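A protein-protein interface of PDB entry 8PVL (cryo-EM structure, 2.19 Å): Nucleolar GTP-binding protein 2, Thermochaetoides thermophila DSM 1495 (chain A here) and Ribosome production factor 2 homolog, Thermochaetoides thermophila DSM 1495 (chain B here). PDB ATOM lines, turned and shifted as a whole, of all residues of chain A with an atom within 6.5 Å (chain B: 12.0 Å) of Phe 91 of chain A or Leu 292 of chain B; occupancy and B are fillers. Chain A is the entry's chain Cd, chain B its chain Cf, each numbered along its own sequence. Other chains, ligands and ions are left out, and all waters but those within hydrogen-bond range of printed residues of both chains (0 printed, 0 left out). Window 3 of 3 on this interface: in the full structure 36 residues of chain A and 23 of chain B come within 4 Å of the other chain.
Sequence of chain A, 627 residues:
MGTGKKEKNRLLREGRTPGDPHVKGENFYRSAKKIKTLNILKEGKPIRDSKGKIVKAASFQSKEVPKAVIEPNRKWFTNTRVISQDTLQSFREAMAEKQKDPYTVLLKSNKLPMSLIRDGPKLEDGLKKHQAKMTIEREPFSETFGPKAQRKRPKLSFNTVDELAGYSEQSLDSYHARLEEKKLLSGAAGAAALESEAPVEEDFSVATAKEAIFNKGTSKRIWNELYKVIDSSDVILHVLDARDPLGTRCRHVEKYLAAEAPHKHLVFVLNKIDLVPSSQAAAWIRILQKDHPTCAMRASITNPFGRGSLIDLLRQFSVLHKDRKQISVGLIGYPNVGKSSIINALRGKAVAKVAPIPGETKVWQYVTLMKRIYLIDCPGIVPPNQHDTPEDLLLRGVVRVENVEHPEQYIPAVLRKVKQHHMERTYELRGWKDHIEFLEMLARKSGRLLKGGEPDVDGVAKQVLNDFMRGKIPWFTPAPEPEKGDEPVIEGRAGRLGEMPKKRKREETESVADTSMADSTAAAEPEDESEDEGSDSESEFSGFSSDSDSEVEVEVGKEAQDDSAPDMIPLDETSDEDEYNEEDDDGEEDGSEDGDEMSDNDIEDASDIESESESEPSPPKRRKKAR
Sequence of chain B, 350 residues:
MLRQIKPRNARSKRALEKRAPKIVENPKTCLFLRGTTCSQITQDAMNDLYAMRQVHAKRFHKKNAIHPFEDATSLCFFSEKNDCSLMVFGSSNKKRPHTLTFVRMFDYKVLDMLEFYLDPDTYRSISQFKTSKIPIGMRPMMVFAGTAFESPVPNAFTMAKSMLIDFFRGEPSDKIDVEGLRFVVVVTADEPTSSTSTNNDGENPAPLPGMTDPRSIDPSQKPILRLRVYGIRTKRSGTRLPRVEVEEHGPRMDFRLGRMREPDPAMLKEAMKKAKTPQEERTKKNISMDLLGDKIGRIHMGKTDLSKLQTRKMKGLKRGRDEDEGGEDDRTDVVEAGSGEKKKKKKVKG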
ATOM      1  N   ILE A  83      -2.830 -28.693  10.611  1.00  0.00           N
ATOM      2  CA  ILE A  83      -3.453 -27.480  11.133  1.00  0.00           C
ATOM      3  C   ILE A  83      -4.929 -27.771  11.381  1.00  0.00           C
ATOM      4  O   ILE A  83      -5.552 -28.556  10.660  1.00  0.00           O
ATOM      5  CB  ILE A  83      -3.230 -26.283  10.175  1.00  0.00           C
ATOM      6  CG1 ILE A  83      -3.679 -24.964  10.811  1.00  0.00           C
ATOM      7  CG2 ILE A  83      -3.898 -26.511   8.822  1.00  0.00           C
ATOM      8  CD1 ILE A  83      -3.119 -23.739  10.130  1.00  0.00           C
ATOM      9  N   ASP A  86      -9.882 -24.372  13.961  1.00  0.00           N
ATOM     10  CA  ASP A  86      -9.867 -23.184  14.812  1.00  0.00           C
ATOM     11  C   ASP A  86      -8.676 -22.288  14.492  1.00  0.00           C
ATOM     12  O   ASP A  86      -8.816 -21.060  14.413  1.00  0.00           O
ATOM     13  CB  ASP A  86      -9.845 -23.599  16.282  1.00  0.00           C
ATOM     14  CG  ASP A  86     -10.767 -24.763  16.570  1.00  0.00           C
ATOM     15  OD1 ASP A  86     -10.699 -25.771  15.835  1.00  0.00           O
ATOM     16  OD2 ASP A  86     -11.557 -24.674  17.534  1.00  0.00           O
ATOM     17  N   THR A  87      -7.498 -22.889  14.303  1.00  0.00           N
ATOM     18  CA  THR A  87      -6.319 -22.128  13.907  1.00  0.00           C
ATOM     19  C   THR A  87      -6.510 -21.505  12.530  1.00  0.00           C
ATOM     20  O   THR A  87      -6.111 -20.355  12.299  1.00  0.00           O
ATOM     21  CB  THR A  87      -5.090 -23.037  13.924  1.00  0.00           C
ATOM     22  OG1 THR A  87      -5.054 -23.764  15.157  1.00  0.00           O
ATOM     23  CG2 THR A  87      -3.825 -22.221  13.806  1.00  0.00           C
ATOM     24  N   LEU A  88      -7.138 -22.245  11.610  1.00  0.00           N
ATOM     25  CA  LEU A  88      -7.439 -21.700  10.289  1.00  0.00           C
ATOM     26  C   LEU A  88      -8.388 -20.510  10.376  1.00  0.00           C
ATOM     27  O   LEU A  88      -8.196 -19.509   9.681  1.00  0.00           O
ATOM     28  CB  LEU A  88      -8.029 -22.785   9.391  1.00  0.00           C
ATOM     29  CG  LEU A  88      -7.026 -23.700   8.689  1.00  0.00           C
ATOM     30  CD1 LEU A  88      -7.748 -24.795   7.928  1.00  0.00           C
ATOM     31  CD2 LEU A  88      -6.138 -22.897   7.759  1.00  0.00           C
ATOM     32  N   GLN A  89      -9.417 -20.601  11.224  1.00  0.00           N
ATOM     33  CA  GLN A  89     -10.366 -19.501  11.377  1.00  0.00           C
ATOM     34  C   GLN A  89      -9.705 -18.272  11.990  1.00  0.00           C
ATOM     35  O   GLN A  89      -9.984 -17.138  11.574  1.00  0.00           O
ATOM     36  CB  GLN A  89     -11.554 -19.949  12.229  1.00  0.00           C
ATOM     37  CG  GLN A  89     -12.886 -19.347  11.809  1.00  0.00           C
ATOM     38  CD  GLN A  89     -13.039 -19.249  10.304  1.00  0.00           C
ATOM     39  OE1 GLN A  89     -13.053 -20.260   9.601  1.00  0.00           O
ATOM     40  NE2 GLN A  89     -13.153 -18.025   9.800  1.00  0.00           N
ATOM     41  N   SER A  90      -8.825 -18.481  12.976  1.00  0.00           N
ATOM     42  CA  SER A  90      -8.081 -17.366  13.556  1.00  0.00           C
ATOM     43  C   SER A  90      -7.194 -16.693  12.516  1.00  0.00           C
ATOM     44  O   SER A  90      -7.131 -15.458  12.443  1.00  0.00           O
ATOM     45  CB  SER A  90      -7.244 -17.851  14.738  1.00  0.00           C
ATOM     46  OG  SER A  90      -8.059 -18.439  15.732  1.00  0.00           O
ATOM     47  N   PHE A  91      -6.519 -17.491  11.683  1.00  0.00           N
ATOM     48  CA  PHE A  91      -5.669 -16.915  10.648  1.00  0.00           C
ATOM     49  C   PHE A  91      -6.483 -16.211   9.568  1.00  0.00           C
ATOM     50  O   PHE A  91      -6.029 -15.203   9.023  1.00  0.00           O
ATOM     51  CB  PHE A  91      -4.779 -17.994  10.037  1.00  0.00           C
ATOM     52  CG  PHE A  91      -3.583 -18.332  10.877  1.00  0.00           C
ATOM     53  CD1 PHE A  91      -2.925 -17.346  11.592  1.00  0.00           C
ATOM     54  CD2 PHE A  91      -3.120 -19.633  10.957  1.00  0.00           C
ATOM     55  CE1 PHE A  91      -1.825 -17.651  12.370  1.00  0.00           C
ATOM     56  CE2 PHE A  91      -2.019 -19.943  11.731  1.00  0.00           C
ATOM     57  CZ  PHE A  91      -1.373 -18.952  12.439  1.00  0.00           C
ATOM     58  N   ARG A  92      -7.682 -16.712   9.255  1.00  0.00           N
ATOM     59  CA  ARG A  92      -8.542 -16.034   8.288  1.00  0.00           C
ATOM     60  C   ARG A  92      -9.028 -14.691   8.819  1.00  0.00           C
ATOM     61  O   ARG A  92      -9.079 -13.704   8.073  1.00  0.00           O
ATOM     62  CB  ARG A  92      -9.731 -16.923   7.925  1.00  0.00           C
ATOM     63  CG  ARG A  92      -9.381 -18.111   7.056  1.00  0.00           C
ATOM     64  CD  ARG A  92     -10.626 -18.789   6.530  1.00  0.00           C
ATOM     65  NE  ARG A  92     -10.332 -20.109   5.987  1.00  0.00           N
ATOM     66  CZ  ARG A  92     -10.748 -21.247   6.524  1.00  0.00           C
ATOM     67  NH1 ARG A  92     -11.490 -21.265   7.619  1.00  0.00           N
ATOM     68  NH2 ARG A  92     -10.411 -22.397   5.948  1.00  0.00           N
ATOM     69  N   GLU A  93      -9.392 -14.634  10.104  1.00  0.00           N
ATOM     70  CA  GLU A  93      -9.788 -13.360  10.701  1.00  0.00           C
ATOM     71  C   GLU A  93      -8.622 -12.376  10.733  1.00  0.00           C
ATOM     72  O   GLU A  93      -8.804 -11.180  10.466  1.00  0.00           O
ATOM     73  CB  GLU A  93     -10.343 -13.590  12.105  1.00  0.00           C
ATOM     74  CG  GLU A  93     -11.683 -14.306  12.124  1.00  0.00           C
ATOM     75  CD  GLU A  93     -11.899 -15.105  13.393  1.00  0.00           C
ATOM     76  OE1 GLU A  93     -10.973 -15.161  14.228  1.00  0.00           O
ATOM     77  OE2 GLU A  93     -12.995 -15.683  13.553  1.00  0.00           O
ATOM     78  N   ALA A  94      -7.417 -12.866  11.043  1.00  0.00           N
ATOM     79  CA  ALA A  94      -6.235 -12.008  11.009  1.00  0.00           C
ATOM     80  C   ALA A  94      -5.940 -11.516   9.595  1.00  0.00           C
ATOM     81  O   ALA A  94      -5.531 -10.364   9.404  1.00  0.00           O
ATOM     82  CB  ALA A  94      -5.033 -12.760  11.575  1.00  0.00           C
ATOM     83  N   MET A  95      -6.129 -12.382   8.597  1.00  0.00           N
ATOM     84  CA  MET A  95      -5.947 -11.996   7.201  1.00  0.00           C
ATOM     85  C   MET A  95      -6.947 -10.926   6.790  1.00  0.00           C
ATOM     86  O   MET A  95      -6.615 -10.015   6.022  1.00  0.00           O
ATOM     87  CB  MET A  95      -6.089 -13.228   6.306  1.00  0.00           C
ATOM     88  CG  MET A  95      -5.477 -13.097   4.923  1.00  0.00           C
ATOM     89  SD  MET A  95      -3.705 -12.793   4.948  1.00  0.00           S
ATOM     90  CE  MET A  95      -3.433 -12.268   3.260  1.00  0.00           C
ATOM     91  N   ALA A  96      -8.185 -11.035   7.272  1.00  0.00           N
ATOM     92  CA  ALA A  96      -9.187 -10.020   6.967  1.00  0.00           C
ATOM     93  C   ALA A  96      -8.862  -8.692   7.641  1.00  0.00           C
ATOM     94  O   ALA A  96      -9.058  -7.626   7.046  1.00  0.00           O
ATOM     95  CB  ALA A  96     -10.572 -10.509   7.388  1.00  0.00           C
ATOM     96  N   LYS A  98      -5.865  -7.537   8.804  1.00  0.00           N
ATOM     97  CA  LYS A  98      -4.503  -7.021   8.693  1.00  0.00           C
ATOM     98  C   LYS A  98      -4.447  -5.749   7.851  1.00  0.00           C
ATOM     99  O   LYS A  98      -5.202  -5.578   6.890  1.00  0.00           O
ATOM    100  CB  LYS A  98      -3.569  -8.091   8.113  1.00  0.00           C
ATOM    101  CG  LYS A  98      -3.789  -8.431   6.642  1.00  0.00           C
ATOM    102  CD  LYS A  98      -2.479  -8.503   5.858  1.00  0.00           C
ATOM    103  CE  LYS A  98      -1.417  -9.309   6.593  1.00  0.00           C
ATOM    104  NZ  LYS A  98      -0.114  -9.302   5.872  1.00  0.00           N
ATOM    105  N   ASN A 110       6.062 -16.644   8.421  1.00  0.00           N
ATOM    106  CA  ASN A 110       5.503 -17.837   9.038  1.00  0.00           C
ATOM    107  C   ASN A 110       5.132 -18.837   7.953  1.00  0.00           C
ATOM    108  O   ASN A 110       4.417 -18.498   7.005  1.00  0.00           O
ATOM    109  CB  ASN A 110       4.276 -17.479   9.874  1.00  0.00           C
ATOM    110  CG  ASN A 110       3.880 -18.580  10.834  1.00  0.00           C
ATOM    111  OD1 ASN A 110       4.635 -19.522  11.064  1.00  0.00           O
ATOM    112  ND2 ASN A 110       2.685 -18.467  11.400  1.00  0.00           N
ATOM    113  N   LEU A 112       2.965 -21.118   6.449  1.00  0.00           N
ATOM    114  CA  LEU A 112       1.533 -21.315   6.592  1.00  0.00           C
ATOM    115  C   LEU A 112       0.950 -21.810   5.279  1.00  0.00           C
ATOM    116  O   LEU A 112       1.469 -21.485   4.205  1.00  0.00           O
ATOM    117  CB  LEU A 112       0.830 -20.010   6.997  1.00  0.00           C
ATOM    118  CG  LEU A 112       1.032 -19.502   8.423  1.00  0.00           C
ATOM    119  CD1 LEU A 112       0.199 -18.259   8.657  1.00  0.00           C
ATOM    120  CD2 LEU A 112       0.680 -20.579   9.427  1.00  0.00           C
ATOM    121  N   PRO A 113      -0.130 -22.592   5.331  1.00  0.00           N
ATOM    122  CA  PRO A 113      -0.858 -22.946   4.095  1.00  0.00           C
ATOM    123  C   PRO A 113      -1.717 -21.778   3.617  1.00  0.00           C
ATOM    124  O   PRO A 113      -2.910 -21.667   3.890  1.00  0.00           O
ATOM    125  CB  PRO A 113      -1.692 -24.153   4.530  1.00  0.00           C
ATOM    126  CG  PRO A 113      -1.911 -23.952   5.986  1.00  0.00           C
ATOM    127  CD  PRO A 113      -0.699 -23.254   6.519  1.00  0.00           C
ATOM    128  N   MET A 114      -1.075 -20.869   2.878  1.00  0.00           N
ATOM    129  CA  MET A 114      -1.695 -19.598   2.521  1.00  0.00           C
ATOM    130  C   MET A 114      -2.854 -19.751   1.546  1.00  0.00           C
ATOM    131  O   MET A 114      -3.680 -18.839   1.447  1.00  0.00           O
ATOM    132  CB  MET A 114      -0.648 -18.650   1.937  1.00  0.00           C
ATOM    133  CG  MET A 114       0.168 -17.912   2.982  1.00  0.00           C
ATOM    134  SD  MET A 114      -0.774 -17.535   4.473  1.00  0.00           S
ATOM    135  CE  MET A 114      -1.566 -16.002   3.998  1.00  0.00           C
ATOM    136  N   ILE A 117      -5.907 -19.847   3.665  1.00  0.00           N
ATOM    137  CA  ILE A 117      -6.077 -18.687   4.524  1.00  0.00           C
ATOM    138  C   ILE A 117      -6.442 -17.442   3.724  1.00  0.00           C
ATOM    139  O   ILE A 117      -7.261 -16.634   4.167  1.00  0.00           O
ATOM    140  CB  ILE A 117      -4.805 -18.453   5.371  1.00  0.00           C
ATOM    141  CG1 ILE A 117      -4.447 -19.724   6.142  1.00  0.00           C
ATOM    142  CG2 ILE A 117      -4.993 -17.299   6.340  1.00  0.00           C
ATOM    143  CD1 ILE A 117      -3.170 -19.621   6.937  1.00  0.00           C
ATOM    144  N   GLU B 281       8.025 -15.979  26.000  1.00  0.00           N
ATOM    145  CA  GLU B 281       9.019 -15.365  25.131  1.00  0.00           C
ATOM    146  C   GLU B 281       9.691 -14.185  25.819  1.00  0.00           C
ATOM    147  O   GLU B 281       9.032 -13.347  26.443  1.00  0.00           O
ATOM    148  CB  GLU B 281       8.373 -14.905  23.823  1.00  0.00           C
ATOM    149  CG  GLU B 281       9.365 -14.360  22.804  1.00  0.00           C
ATOM    150  CD  GLU B 281       8.708 -13.523  21.726  1.00  0.00           C
ATOM    151  OE1 GLU B 281       7.739 -14.005  21.103  1.00  0.00           O
ATOM    152  OE2 GLU B 281       9.164 -12.384  21.498  1.00  0.00           O
ATOM    153  N   SER B 288       8.487  -8.031  17.284  1.00  0.00           N
ATOM    154  CA  SER B 288       7.225  -8.579  17.759  1.00  0.00           C
ATOM    155  C   SER B 288       6.742  -9.630  16.770  1.00  0.00           C
ATOM    156  O   SER B 288       7.388  -9.909  15.757  1.00  0.00           O
ATOM    157  CB  SER B 288       6.174  -7.480  17.957  1.00  0.00           C
ATOM    158  OG  SER B 288       5.653  -7.036  16.718  1.00  0.00           O
ATOM    159  N   MET B 289       5.599 -10.225  17.081  1.00  0.00           N
ATOM    160  CA  MET B 289       4.941 -11.190  16.216  1.00  0.00           C
ATOM    161  C   MET B 289       3.579 -10.638  15.835  1.00  0.00           C
ATOM    162  O   MET B 289       2.836 -10.168  16.703  1.00  0.00           O
ATOM    163  CB  MET B 289       4.784 -12.536  16.921  1.00  0.00           C
ATOM    164  CG  MET B 289       4.290 -13.653  16.034  1.00  0.00           C
ATOM    165  SD  MET B 289       4.691 -15.258  16.731  1.00  0.00           S
ATOM    166  CE  MET B 289       3.285 -15.524  17.803  1.00  0.00           C
ATOM    167  N   ASP B 290       3.244 -10.690  14.549  1.00  0.00           N
ATOM    168  CA  ASP B 290       1.935 -10.199  14.136  1.00  0.00           C
ATOM    169  C   ASP B 290       0.892 -11.294  14.369  1.00  0.00           C
ATOM    170  O   ASP B 290       1.184 -12.359  14.919  1.00  0.00           O
ATOM    171  CB  ASP B 290       1.975  -9.687  12.694  1.00  0.00           C
ATOM    172  CG  ASP B 290       2.185 -10.786  11.666  1.00  0.00           C
ATOM    173  OD1 ASP B 290       2.583 -11.909  12.029  1.00  0.00           O
ATOM    174  OD2 ASP B 290       1.949 -10.513  10.471  1.00  0.00           O
ATOM    175  N   LEU B 291      -0.344 -11.050  13.944  1.00  0.00           N
ATOM    176  CA  LEU B 291      -1.406 -12.022  14.167  1.00  0.00           C
ATOM    177  C   LEU B 291      -1.341 -13.208  13.213  1.00  0.00           C
ATOM    178  O   LEU B 291      -2.027 -14.208  13.451  1.00  0.00           O
ATOM    179  CB  LEU B 291      -2.769 -11.337  14.061  1.00  0.00           C
ATOM    180  CG  LEU B 291      -3.162 -10.484  15.269  1.00  0.00           C
ATOM    181  CD1 LEU B 291      -4.536  -9.867  15.072  1.00  0.00           C
ATOM    182  CD2 LEU B 291      -3.120 -11.311  16.544  1.00  0.00           C
ATOM    183  N   LEU B 292      -0.544 -13.129  12.152  1.00  0.00           N
ATOM    184  CA  LEU B 292      -0.324 -14.258  11.261  1.00  0.00           C
ATOM    185  C   LEU B 292       0.937 -15.044  11.595  1.00  0.00           C
ATOM    186  O   LEU B 292       1.265 -15.992  10.877  1.00  0.00           O
ATOM    187  CB  LEU B 292      -0.261 -13.783   9.807  1.00  0.00           C
ATOM    188  CG  LEU B 292      -1.608 -13.670   9.097  1.00  0.00           C
ATOM    189  CD1 LEU B 292      -1.473 -12.824   7.850  1.00  0.00           C
ATOM    190  CD2 LEU B 292      -2.147 -15.048   8.755  1.00  0.00           C
ATOM    191  N   GLY B 293       1.644 -14.680  12.660  1.00  0.00           N
ATOM    192  CA  GLY B 293       2.839 -15.385  13.064  1.00  0.00           C
ATOM    193  C   GLY B 293       4.130 -14.891  12.451  1.00  0.00           C
ATOM    194  O   GLY B 293       5.189 -15.459  12.745  1.00  0.00           O
ATOM    195  N   ASP B 294       4.085 -13.860  11.611  1.00  0.00           N
ATOM    196  CA  ASP B 294       5.306 -13.306  11.044  1.00  0.00           C
ATOM    197  C   ASP B 294       6.060 -12.496  12.090  1.00  0.00           C
ATOM    198  O   ASP B 294       5.462 -11.780  12.901  1.00  0.00           O
ATOM    199  CB  ASP B 294       4.987 -12.418   9.842  1.00  0.00           C
ATOM    200  CG  ASP B 294       4.392 -13.190   8.686  1.00  0.00           C
ATOM    201  OD1 ASP B 294       4.560 -14.424   8.641  1.00  0.00           O
ATOM    202  OD2 ASP B 294       3.755 -12.559   7.819  1.00  0.00           O
ATOM    203  N   LYS B 295       7.386 -12.616  12.062  1.00  0.00           N
ATOM    204  CA  LYS B 295       8.252 -11.787  12.885  1.00  0.00           C
ATOM    205  C   LYS B 295       8.381 -10.410  12.248  1.00  0.00           C
ATOM    206  O   LYS B 295       8.755 -10.289  11.078  1.00  0.00           O
ATOM    207  CB  LYS B 295       9.624 -12.441  13.043  1.00  0.00           C
ATOM    208  CG  LYS B 295      10.515 -11.779  14.074  1.00  0.00           C
ATOM    209  CD  LYS B 295      11.907 -12.387  14.078  1.00  0.00           C
ATOM    210  CE  LYS B 295      11.879 -13.827  14.551  1.00  0.00           C
ATOM    211  NZ  LYS B 295      13.223 -14.459  14.491  1.00  0.00           N
ATOM    212  N   ILE B 296       8.072  -9.373  13.019  1.00  0.00           N
ATOM    213  CA  ILE B 296       7.948  -8.012  12.520  1.00  0.00           C
ATOM    214  C   ILE B 296       8.921  -7.130  13.286  1.00  0.00           C
ATOM    215  O   ILE B 296       8.990  -7.196  14.520  1.00  0.00           O
ATOM    216  CB  ILE B 296       6.502  -7.497  12.663  1.00  0.00           C
ATOM    217  CG1 ILE B 296       5.542  -8.360  11.841  1.00  0.00           C
ATOM    218  CG2 ILE B 296       6.390  -6.050  12.240  1.00  0.00           C
ATOM    219  CD1 ILE B 296       5.880  -8.424  10.373  1.00  0.00           C
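No residue of chain B comes within 4 Å of Leu 88 of chain A.
Of chain B, only Leu 291 (3.6 Å) and Leu 292 (3.7 Å) come within 4 Å of Phe 91 of chain A.
Of the printed residues of chain B, Ala 94 of chain A touches Leu 291.
Met 95 of chain A touches just one residue of chain B: Leu 292 (3.7 Å).
Printed residues of chain B within 4 Å of Lys 98 of chain A: Leu 292 (3.7 Å).
Of chain B, only Leu 292, Gly 293 and Asp 294 come within 4 Å of Asn 110 of chain A.
Met 114 of chain A touches none of the printed residues of chain B.
Ile 117 of chain A touches none of the printed residues of chain B.
Of the printed residues of chain A, Leu 292 of chain B touches Phe 91 (3.7 Å), Met 95 (3.7 Å), Lys 98 (3.7 Å), Asn 110 (2.9 Å) and Leu 112 (3.3 Å).
Printed residues of chain A within 4 Å of Gly 293 of chain B: Asn 110.
The nearest residue of chain B that does not touch Phe 91 of chain A is Gly 293 of chain B (4.6 Å).
The nearest residue of chain A that does not touch Leu 292 of chain B is Ala 94 of chain A (4.3 Å).
The nearest printed residue of chain A that does not touch Gly 293 of chain B is Phe 91 of chain A (4.6 Å).
O of Leu 291 of chain B touches CE1 of Phe 91 of chain A, 3.6 Å away.
Leu 292 of chain B touches Phe 91 of chain A.
Ala 94 of chain A touches Leu 291 of chain B (CB to CB, 3.7 Å).
SD of Met 95 of chain A touches CD1 of Leu 292 of chain B, at 3.7 Å.
CD1 of Leu 292 of chain B touches CE of Lys 98 of chain A, at 3.7 Å.
Asn 110 of chain A touches Gly 293 of chain B.
O of Leu 292 of chain B touches CD1 of Leu 112 of chain A (3.3 Å).
Of the 10 printed residues of chain B, 4 touch a printed residue of chain A.
Hydrophobic or aromatic side chains of chain B within 4 Å of the printed part of chain A: Leu 291 and Leu 292.
Of the 18 printed residues of chain A, 6 touch a printed residue of chain B.
Hydrophobic or aromatic side chains of chain A that line the printed part of chain B: Phe 91, Ala 94, Met 95 and Leu 112.
Among the printed residues, 9 pairs touch across the chains.
The side-chain carboxylate of Asp 294 of chain B is in hydrogen-bond range of the backbone NH of Asn 110 of chain A, 2.7 Å away.
The side-chain amide nitrogen of Asn 110 of chain A sits at hydrogen-bond distance from the backbone carbonyl oxygen of Leu 292 of chain B (2.9 Å).
The side-chain carboxylate (OD1) of Asp 290 of chain B sits at hydrogen-bond distance from the backbone NH (N) of Gly 293 of chain B, 3.0 Å away.
The side-chain carboxylate (OD1) of Asp 290 of chain B sits close to the backbone NH (N) of Leu 292 of chain B.
The side-chain carboxylate of Asp 290 of chain B lies within hydrogen-bond range of the backbone NH of Asp 294 of chain B, 2.5 Å away.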
